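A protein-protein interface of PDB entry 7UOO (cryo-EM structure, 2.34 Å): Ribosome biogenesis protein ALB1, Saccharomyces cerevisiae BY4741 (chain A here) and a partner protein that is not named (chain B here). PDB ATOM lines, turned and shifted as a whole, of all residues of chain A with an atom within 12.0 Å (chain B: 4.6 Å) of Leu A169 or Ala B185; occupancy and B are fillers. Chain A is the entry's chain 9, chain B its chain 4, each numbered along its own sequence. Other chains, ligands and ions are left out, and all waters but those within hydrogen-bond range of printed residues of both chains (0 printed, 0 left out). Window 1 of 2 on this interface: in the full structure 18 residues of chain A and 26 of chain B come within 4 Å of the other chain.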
ATOM      1  N   GLN A 165      28.127  11.775   4.284  1.00  0.00           N
ATOM      2  CA  GLN A 165      27.963  11.524   2.857  1.00  0.00           C
ATOM      3  C   GLN A 165      26.777  12.294   2.286  1.00  0.00           C
ATOM      4  O   GLN A 165      26.914  13.440   1.860  1.00  0.00           O
ATOM      5  CB  GLN A 165      27.789  10.027   2.595  1.00  0.00           C
ATOM      6  CG  GLN A 165      29.075   9.231   2.707  1.00  0.00           C
ATOM      7  CD  GLN A 165      30.092   9.631   1.658  1.00  0.00           C
ATOM      8  OE1 GLN A 165      29.736   9.986   0.535  1.00  0.00           O
ATOM      9  NE2 GLN A 165      31.368   9.583   2.022  1.00  0.00           N
ATOM     10  N   GLY A 166      25.612  11.653   2.286  1.00  0.00           N
ATOM     11  CA  GLY A 166      24.407  12.258   1.756  1.00  0.00           C
ATOM     12  C   GLY A 166      23.660  11.328   0.824  1.00  0.00           C
ATOM     13  O   GLY A 166      23.408  10.169   1.164  1.00  0.00           O
ATOM     14  N   THR A 167      23.298  11.826  -0.355  1.00  0.00           N
ATOM     15  CA  THR A 167      22.674  10.996  -1.373  1.00  0.00           C
ATOM     16  C   THR A 167      22.997  11.574  -2.742  1.00  0.00           C
ATOM     17  O   THR A 167      23.291  12.765  -2.877  1.00  0.00           O
ATOM     18  CB  THR A 167      21.156  10.890  -1.180  1.00  0.00           C
ATOM     19  OG1 THR A 167      20.603  10.038  -2.189  1.00  0.00           O
ATOM     20  CG2 THR A 167      20.511  12.254  -1.280  1.00  0.00           C
ATOM     21  N   THR A 168      22.956  10.712  -3.754  1.00  0.00           N
ATOM     22  CA  THR A 168      23.224  11.109  -5.128  1.00  0.00           C
ATOM     23  C   THR A 168      22.338  10.292  -6.054  1.00  0.00           C
ATOM     24  O   THR A 168      22.297   9.063  -5.951  1.00  0.00           O
ATOM     25  CB  THR A 168      24.699  10.904  -5.495  1.00  0.00           C
ATOM     26  OG1 THR A 168      25.530  11.639  -4.586  1.00  0.00           O
ATOM     27  CG2 THR A 168      24.970  11.381  -6.915  1.00  0.00           C
ATOM     28  N   LEU A 169      21.627  10.975  -6.946  1.00  0.00           N
ATOM     29  CA  LEU A 169      20.782  10.327  -7.936  1.00  0.00           C
ATOM     30  C   LEU A 169      21.172  10.821  -9.321  1.00  0.00           C
ATOM     31  O   LEU A 169      21.620  11.958  -9.485  1.00  0.00           O
ATOM     32  CB  LEU A 169      19.293  10.599  -7.677  1.00  0.00           C
ATOM     33  CG  LEU A 169      18.746  10.168  -6.315  1.00  0.00           C
ATOM     34  CD1 LEU A 169      17.263  10.482  -6.212  1.00  0.00           C
ATOM     35  CD2 LEU A 169      18.997   8.688  -6.073  1.00  0.00           C
ATOM     36  N   GLY A 170      21.009   9.953 -10.312  1.00  0.00           N
ATOM     37  CA  GLY A 170      21.369  10.298 -11.669  1.00  0.00           C
ATOM     38  C   GLY A 170      22.867  10.254 -11.904  1.00  0.00           C
ATOM     39  O   GLY A 170      23.645   9.704 -11.121  1.00  0.00           O
ATOM     40  N   GLY A 171      23.271  10.854 -13.021  1.00  0.00           N
ATOM     41  CA  GLY A 171      24.660  10.882 -13.409  1.00  0.00           C
ATOM     42  C   GLY A 171      24.945  11.930 -14.463  1.00  0.00           C
ATOM     43  O   GLY A 171      24.041  12.616 -14.950  1.00  0.00           O
ATOM     44  N   PRO A 172      26.217  12.068 -14.843  1.00  0.00           N
ATOM     45  CA  PRO A 172      26.595  13.112 -15.807  1.00  0.00           C
ATOM     46  C   PRO A 172      26.133  12.818 -17.226  1.00  0.00           C
ATOM     47  O   PRO A 172      26.943  12.483 -18.096  1.00  0.00           O
ATOM     48  CB  PRO A 172      28.124  13.132 -15.710  1.00  0.00           C
ATOM     49  CG  PRO A 172      28.483  11.752 -15.283  1.00  0.00           C
ATOM     50  CD  PRO A 172      27.385  11.315 -14.357  1.00  0.00           C
ATOM     51  N   PHE A 173      24.832  12.948 -17.468  1.00  0.00           N
ATOM     52  CA  PHE A 173      24.266  12.774 -18.798  1.00  0.00           C
ATOM     53  C   PHE A 173      22.918  13.479 -18.837  1.00  0.00           C
ATOM     54  O   PHE A 173      22.353  13.838 -17.802  1.00  0.00           O
ATOM     55  CB  PHE A 173      24.128  11.293 -19.169  1.00  0.00           C
ATOM     56  CG  PHE A 173      23.356  10.481 -18.166  1.00  0.00           C
ATOM     57  CD1 PHE A 173      21.982  10.337 -18.277  1.00  0.00           C
ATOM     58  CD2 PHE A 173      24.006   9.853 -17.116  1.00  0.00           C
ATOM     59  CE1 PHE A 173      21.273   9.592 -17.355  1.00  0.00           C
ATOM     60  CE2 PHE A 173      23.302   9.107 -16.194  1.00  0.00           C
ATOM     61  CZ  PHE A 173      21.935   8.975 -16.314  1.00  0.00           C
ATOM     62  N   PHE A 174      22.412  13.675 -20.049  1.00  0.00           N
ATOM     63  CA  PHE A 174      21.078  14.231 -20.232  1.00  0.00           C
ATOM     64  C   PHE A 174      20.135  13.124 -20.678  1.00  0.00           C
ATOM     65  O   PHE A 174      20.223  12.672 -21.830  1.00  0.00           O
ATOM     66  CB  PHE A 174      21.094  15.366 -21.255  1.00  0.00           C
ATOM     67  CG  PHE A 174      21.871  16.571 -20.813  1.00  0.00           C
ATOM     68  CD1 PHE A 174      21.419  17.353 -19.764  1.00  0.00           C
ATOM     69  CD2 PHE A 174      23.042  16.933 -21.455  1.00  0.00           C
ATOM     70  CE1 PHE A 174      22.124  18.468 -19.359  1.00  0.00           C
ATOM     71  CE2 PHE A 174      23.753  18.046 -21.053  1.00  0.00           C
ATOM     72  CZ  PHE A 174      23.294  18.815 -20.003  1.00  0.00           C
ATOM     73  N   PRO A 175      19.227  12.648 -19.812  1.00  0.00           N
ATOM     74  CA  PRO A 175      18.270  11.582 -20.132  1.00  0.00           C
ATOM     75  C   PRO A 175      17.322  11.953 -21.268  1.00  0.00           C
ATOM     76  O   PRO A 175      17.573  11.556 -22.406  1.00  0.00           O
ATOM     77  CB  PRO A 175      17.495  11.402 -18.822  1.00  0.00           C
ATOM     78  CG  PRO A 175      18.402  11.928 -17.768  1.00  0.00           C
ATOM     79  CD  PRO A 175      19.132  13.067 -18.403  1.00  0.00           C
ATOM     80  N   ALA B 181      17.756  19.952  -4.856  1.00  0.00           N
ATOM     81  CA  ALA B 181      18.209  18.566  -4.866  1.00  0.00           C
ATOM     82  C   ALA B 181      17.549  17.765  -3.752  1.00  0.00           C
ATOM     83  O   ALA B 181      17.180  16.600  -3.951  1.00  0.00           O
ATOM     84  CB  ALA B 181      19.732  18.510  -4.742  1.00  0.00           C
ATOM     85  N   ASP B 182      17.386  18.378  -2.575  1.00  0.00           N
ATOM     86  CA  ASP B 182      16.682  17.713  -1.480  1.00  0.00           C
ATOM     87  C   ASP B 182      15.252  17.365  -1.881  1.00  0.00           C
ATOM     88  O   ASP B 182      14.778  16.249  -1.636  1.00  0.00           O
ATOM     89  CB  ASP B 182      16.676  18.603  -0.235  1.00  0.00           C
ATOM     90  CG  ASP B 182      18.058  19.108   0.137  1.00  0.00           C
ATOM     91  OD1 ASP B 182      19.050  18.408  -0.147  1.00  0.00           O
ATOM     92  OD2 ASP B 182      18.154  20.209   0.717  1.00  0.00           O
ATOM     93  N   ALA B 183      14.557  18.313  -2.514  1.00  0.00           N
ATOM     94  CA  ALA B 183      13.171  18.088  -2.917  1.00  0.00           C
ATOM     95  C   ALA B 183      13.065  16.997  -3.978  1.00  0.00           C
ATOM     96  O   ALA B 183      12.183  16.133  -3.900  1.00  0.00           O
ATOM     97  CB  ALA B 183      12.556  19.393  -3.422  1.00  0.00           C
ATOM     98  N   VAL B 184      13.956  17.022  -4.974  1.00  0.00           N
ATOM     99  CA  VAL B 184      13.929  16.012  -6.032  1.00  0.00           C
ATOM    100  C   VAL B 184      14.206  14.627  -5.458  1.00  0.00           C
ATOM    101  O   VAL B 184      13.516  13.651  -5.792  1.00  0.00           O
ATOM    102  CB  VAL B 184      14.925  16.377  -7.149  1.00  0.00           C
ATOM    103  CG1 VAL B 184      15.064  15.233  -8.138  1.00  0.00           C
ATOM    104  CG2 VAL B 184      14.472  17.632  -7.871  1.00  0.00           C
ATOM    105  N   ALA B 185      15.212  14.518  -4.583  1.00  0.00           N
ATOM    106  CA  ALA B 185      15.531  13.229  -3.976  1.00  0.00           C
ATOM    107  C   ALA B 185      14.379  12.715  -3.125  1.00  0.00           C
ATOM    108  O   ALA B 185      14.031  11.528  -3.190  1.00  0.00           O
ATOM    109  CB  ALA B 185      16.804  13.346  -3.139  1.00  0.00           C
ATOM    110  N   ALA B 186      13.766  13.597  -2.330  1.00  0.00           N
ATOM    111  CA  ALA B 186      12.642  13.192  -1.493  1.00  0.00           C
ATOM    112  C   ALA B 186      11.478  12.697  -2.341  1.00  0.00           C
ATOM    113  O   ALA B 186      10.886  11.652  -2.045  1.00  0.00           O
ATOM    114  CB  ALA B 186      12.205  14.358  -0.608  1.00  0.00           C
ATOM    115  N   ALA B 187      11.153  13.424  -3.415  1.00  0.00           N
ATOM    116  CA  ALA B 187      10.045  13.019  -4.275  1.00  0.00           C
ATOM    117  C   ALA B 187      10.318  11.677  -4.944  1.00  0.00           C
ATOM    118  O   ALA B 187       9.445  10.800  -4.967  1.00  0.00           O
ATOM    119  CB  ALA B 187       9.775  14.099  -5.324  1.00  0.00           C
ATOM    120  N   HIS B 188      11.530  11.491  -5.475  1.00  0.00           N
ATOM    121  CA  HIS B 188      11.868  10.245  -6.160  1.00  0.00           C
ATOM    122  C   HIS B 188      11.819   9.054  -5.208  1.00  0.00           C
ATOM    123  O   HIS B 188      11.210   8.015  -5.515  1.00  0.00           O
ATOM    124  CB  HIS B 188      13.253  10.377  -6.797  1.00  0.00           C
ATOM    125  CG  HIS B 188      13.641   9.219  -7.661  1.00  0.00           C
ATOM    126  ND1 HIS B 188      14.576   8.283  -7.275  1.00  0.00           N
ATOM    127  CD2 HIS B 188      13.231   8.853  -8.898  1.00  0.00           C
ATOM    128  CE1 HIS B 188      14.720   7.386  -8.234  1.00  0.00           C
ATOM    129  NE2 HIS B 188      13.916   7.709  -9.231  1.00  0.00           N
ATOM    130  N   ILE B 189      12.436   9.195  -4.032  1.00  0.00           N
ATOM    131  CA  ILE B 189      12.489   8.088  -3.083  1.00  0.00           C
ATOM    132  C   ILE B 189      11.102   7.781  -2.531  1.00  0.00           C
ATOM    133  O   ILE B 189      10.738   6.610  -2.360  1.00  0.00           O
ATOM    134  CB  ILE B 189      13.503   8.399  -1.968  1.00  0.00           C
ATOM    135  CG1 ILE B 189      14.907   8.495  -2.562  1.00  0.00           C
ATOM    136  CG2 ILE B 189      13.463   7.339  -0.876  1.00  0.00           C
ATOM    137  CD1 ILE B 189      15.975   8.810  -1.557  1.00  0.00           C
ATOM    138  N   TYR B 234      14.475  14.266   4.612  1.00  0.00           N
ATOM    139  CA  TYR B 234      15.091  15.098   3.585  1.00  0.00           C
ATOM    140  C   TYR B 234      14.812  16.585   3.763  1.00  0.00           C
ATOM    141  O   TYR B 234      15.177  17.376   2.886  1.00  0.00           O
ATOM    142  CB  TYR B 234      14.651  14.635   2.198  1.00  0.00           C
ATOM    143  CG  TYR B 234      15.541  13.546   1.663  1.00  0.00           C
ATOM    144  CD1 TYR B 234      16.842  13.827   1.276  1.00  0.00           C
ATOM    145  CD2 TYR B 234      15.096  12.235   1.566  1.00  0.00           C
ATOM    146  CE1 TYR B 234      17.671  12.842   0.798  1.00  0.00           C
ATOM    147  CE2 TYR B 234      15.921  11.239   1.088  1.00  0.00           C
ATOM    148  CZ  TYR B 234      17.209  11.551   0.704  1.00  0.00           C
ATOM    149  OH  TYR B 234      18.044  10.571   0.225  1.00  0.00           O
ATOM    150  N   PRO B 534      15.755   9.730 -13.195  1.00  0.00           N
ATOM    151  CA  PRO B 534      16.113  10.876 -12.350  1.00  0.00           C
ATOM    152  C   PRO B 534      17.301  11.653 -12.895  1.00  0.00           C
ATOM    153  O   PRO B 534      18.195  11.104 -13.543  1.00  0.00           O
ATOM    154  CB  PRO B 534      16.445  10.229 -11.001  1.00  0.00           C
ATOM    155  CG  PRO B 534      16.851   8.837 -11.345  1.00  0.00           C
ATOM    156  CD  PRO B 534      16.006   8.445 -12.522  1.00  0.00           C
ATOM    157  N   SER B 535      17.296  12.954 -12.616  1.00  0.00           N
ATOM    158  CA  SER B 535      18.353  13.848 -13.058  1.00  0.00           C
ATOM    159  C   SER B 535      19.556  13.764 -12.121  1.00  0.00           C
ATOM    160  O   SER B 535      19.523  13.115 -11.074  1.00  0.00           O
ATOM    161  CB  SER B 535      17.839  15.286 -13.135  1.00  0.00           C
ATOM    162  OG  SER B 535      16.819  15.417 -14.108  1.00  0.00           O
ATOM    163  N   TRP B 536      20.633  14.446 -12.511  1.00  0.00           N
ATOM    164  CA  TRP B 536      21.888  14.428 -11.761  1.00  0.00           C
ATOM    165  C   TRP B 536      21.785  15.412 -10.604  1.00  0.00           C
ATOM    166  O   TRP B 536      21.931  16.622 -10.786  1.00  0.00           O
ATOM    167  CB  TRP B 536      23.059  14.777 -12.671  1.00  0.00           C
ATOM    168  CG  TRP B 536      24.399  14.519 -12.061  1.00  0.00           C
ATOM    169  CD1 TRP B 536      24.666  13.757 -10.961  1.00  0.00           C
ATOM    170  CD2 TRP B 536      25.660  15.025 -12.513  1.00  0.00           C
ATOM    171  NE1 TRP B 536      26.014  13.755 -10.703  1.00  0.00           N
ATOM    172  CE2 TRP B 536      26.647  14.525 -11.642  1.00  0.00           C
ATOM    173  CE3 TRP B 536      26.049  15.852 -13.571  1.00  0.00           C
ATOM    174  CZ2 TRP B 536      27.998  14.826 -11.796  1.00  0.00           C
ATOM    175  CZ3 TRP B 536      27.389  16.147 -13.724  1.00  0.00           C
ATOM    176  CH2 TRP B 536      28.348  15.636 -12.840  1.00  0.00           C
ATOM    177  N   ILE B 537      21.539  14.895  -9.400  1.00  0.00           N
ATOM    178  CA  ILE B 537      21.425  15.718  -8.206  1.00  0.00           C
ATOM    179  C   ILE B 537      22.359  15.170  -7.138  1.00  0.00           C
ATOM    180  O   ILE B 537      22.765  14.007  -7.166  1.00  0.00           O
ATOM    181  CB  ILE B 537      19.981  15.780  -7.660  1.00  0.00           C
ATOM    182  CG1 ILE B 537      19.520  14.389  -7.222  1.00  0.00           C
ATOM    183  CG2 ILE B 537      19.035  16.363  -8.697  1.00  0.00           C
ATOM    184  CD1 ILE B 537      18.240  14.391  -6.429  1.00  0.00           C
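N of Ile B537 is in hydrogen-bond range of O of Leu A169 (2.9 Å). The backbone carbonyl oxygen (O) of Leu A169 lies close to the backbone carbonyl oxygen (O) of Ser B535, 2.9 Å away.
Tyr B234 touches Thr A167. O of Ile B537 touches CG2 of Thr A168 (3.4 Å). CA of Ala B185 touches CD1 of Leu A169 (3.9 Å). His B188 touches Leu A169 (ND1 to CD1, 3.6 Å). Trp B536 touches Leu A169 (CA to O, 3.4 Å). CA of Gly A170 touches O of Pro B534 (3.8 Å). Gly A170 touches Ser B535 (CA to O, 3.4 Å). Gly A171 touches Trp B536 (O to CB, 3.3 Å). CE3 of Trp B536 touches CA of Pro A172, 3.6 Å away.
Of chain B, only Ala B185 (3.9 Å), His B188 (3.6 Å), Ser B535 (2.9 Å), Trp B536 (3.4 Å) and Ile B537 (2.9 Å) come within 4 Å of Leu A169. No residue of chain A comes within 4 Å of Ala B181. No residue of chain A comes within 4 Å of Ala B183. No residue of chain A comes within 4 Å of Val B184. No residue of chain A comes within 4 Å of Ala B186. Of chain A, only Leu A169 (3.6 Å) comes within 4 Å of His B188. Printed residues of chain A within 4 Å of Tyr B234: Thr A167. Printed residues of chain A within 4 Å of Pro B534: Gly A170 (3.8 Å). Of chain A, only Leu A169 (2.9 Å) and Gly A170 (3.4 Å) come within 4 Å of Ser B535. Printed residues of chain B within 4 Å of Thr A168: Ile B537. Printed residues of chain B within 4 Å of Pro A172: Trp B536. Printed residues of chain B within 4 Å of Gly A170: Pro B534 (3.8 Å) and Ser B535 (3.4 Å). Of the printed residues of chain A, Trp B536 touches Leu A169 (3.4 Å), Gly A171 (3.3 Å) and Pro A172 (3.6 Å). Printed residues of chain B within 4 Å of Thr A167: Tyr B234. The nearest residue of chain A that does not touch Ala B185 is Thr A167 (4.3 Å).
Of the 14 printed residues of chain B, 7 touch a printed residue of chain A. Printed residues of chain B that touch a printed residue of chain A: Ala B185, His B188, Tyr B234, Pro B534, Ser B535, Trp B536 and Ile B537. Hydrophobic or aromatic side chains of chain B within 4 Å of the printed part of chain A: His B188, Tyr B234, Trp B536 and Ile B537. Of the 11 printed residues of chain A, 6 touch a printed residue of chain B. Printed residues of chain A that touch a printed residue of chain B: Thr A167, Thr A168, Leu A169, Gly A170, Gly A171 and Pro A172. Among the printed residues, no Asp or Glu carboxylate lies within 4 Å of a Lys or Arg side-chain nitrogen of the other chain.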
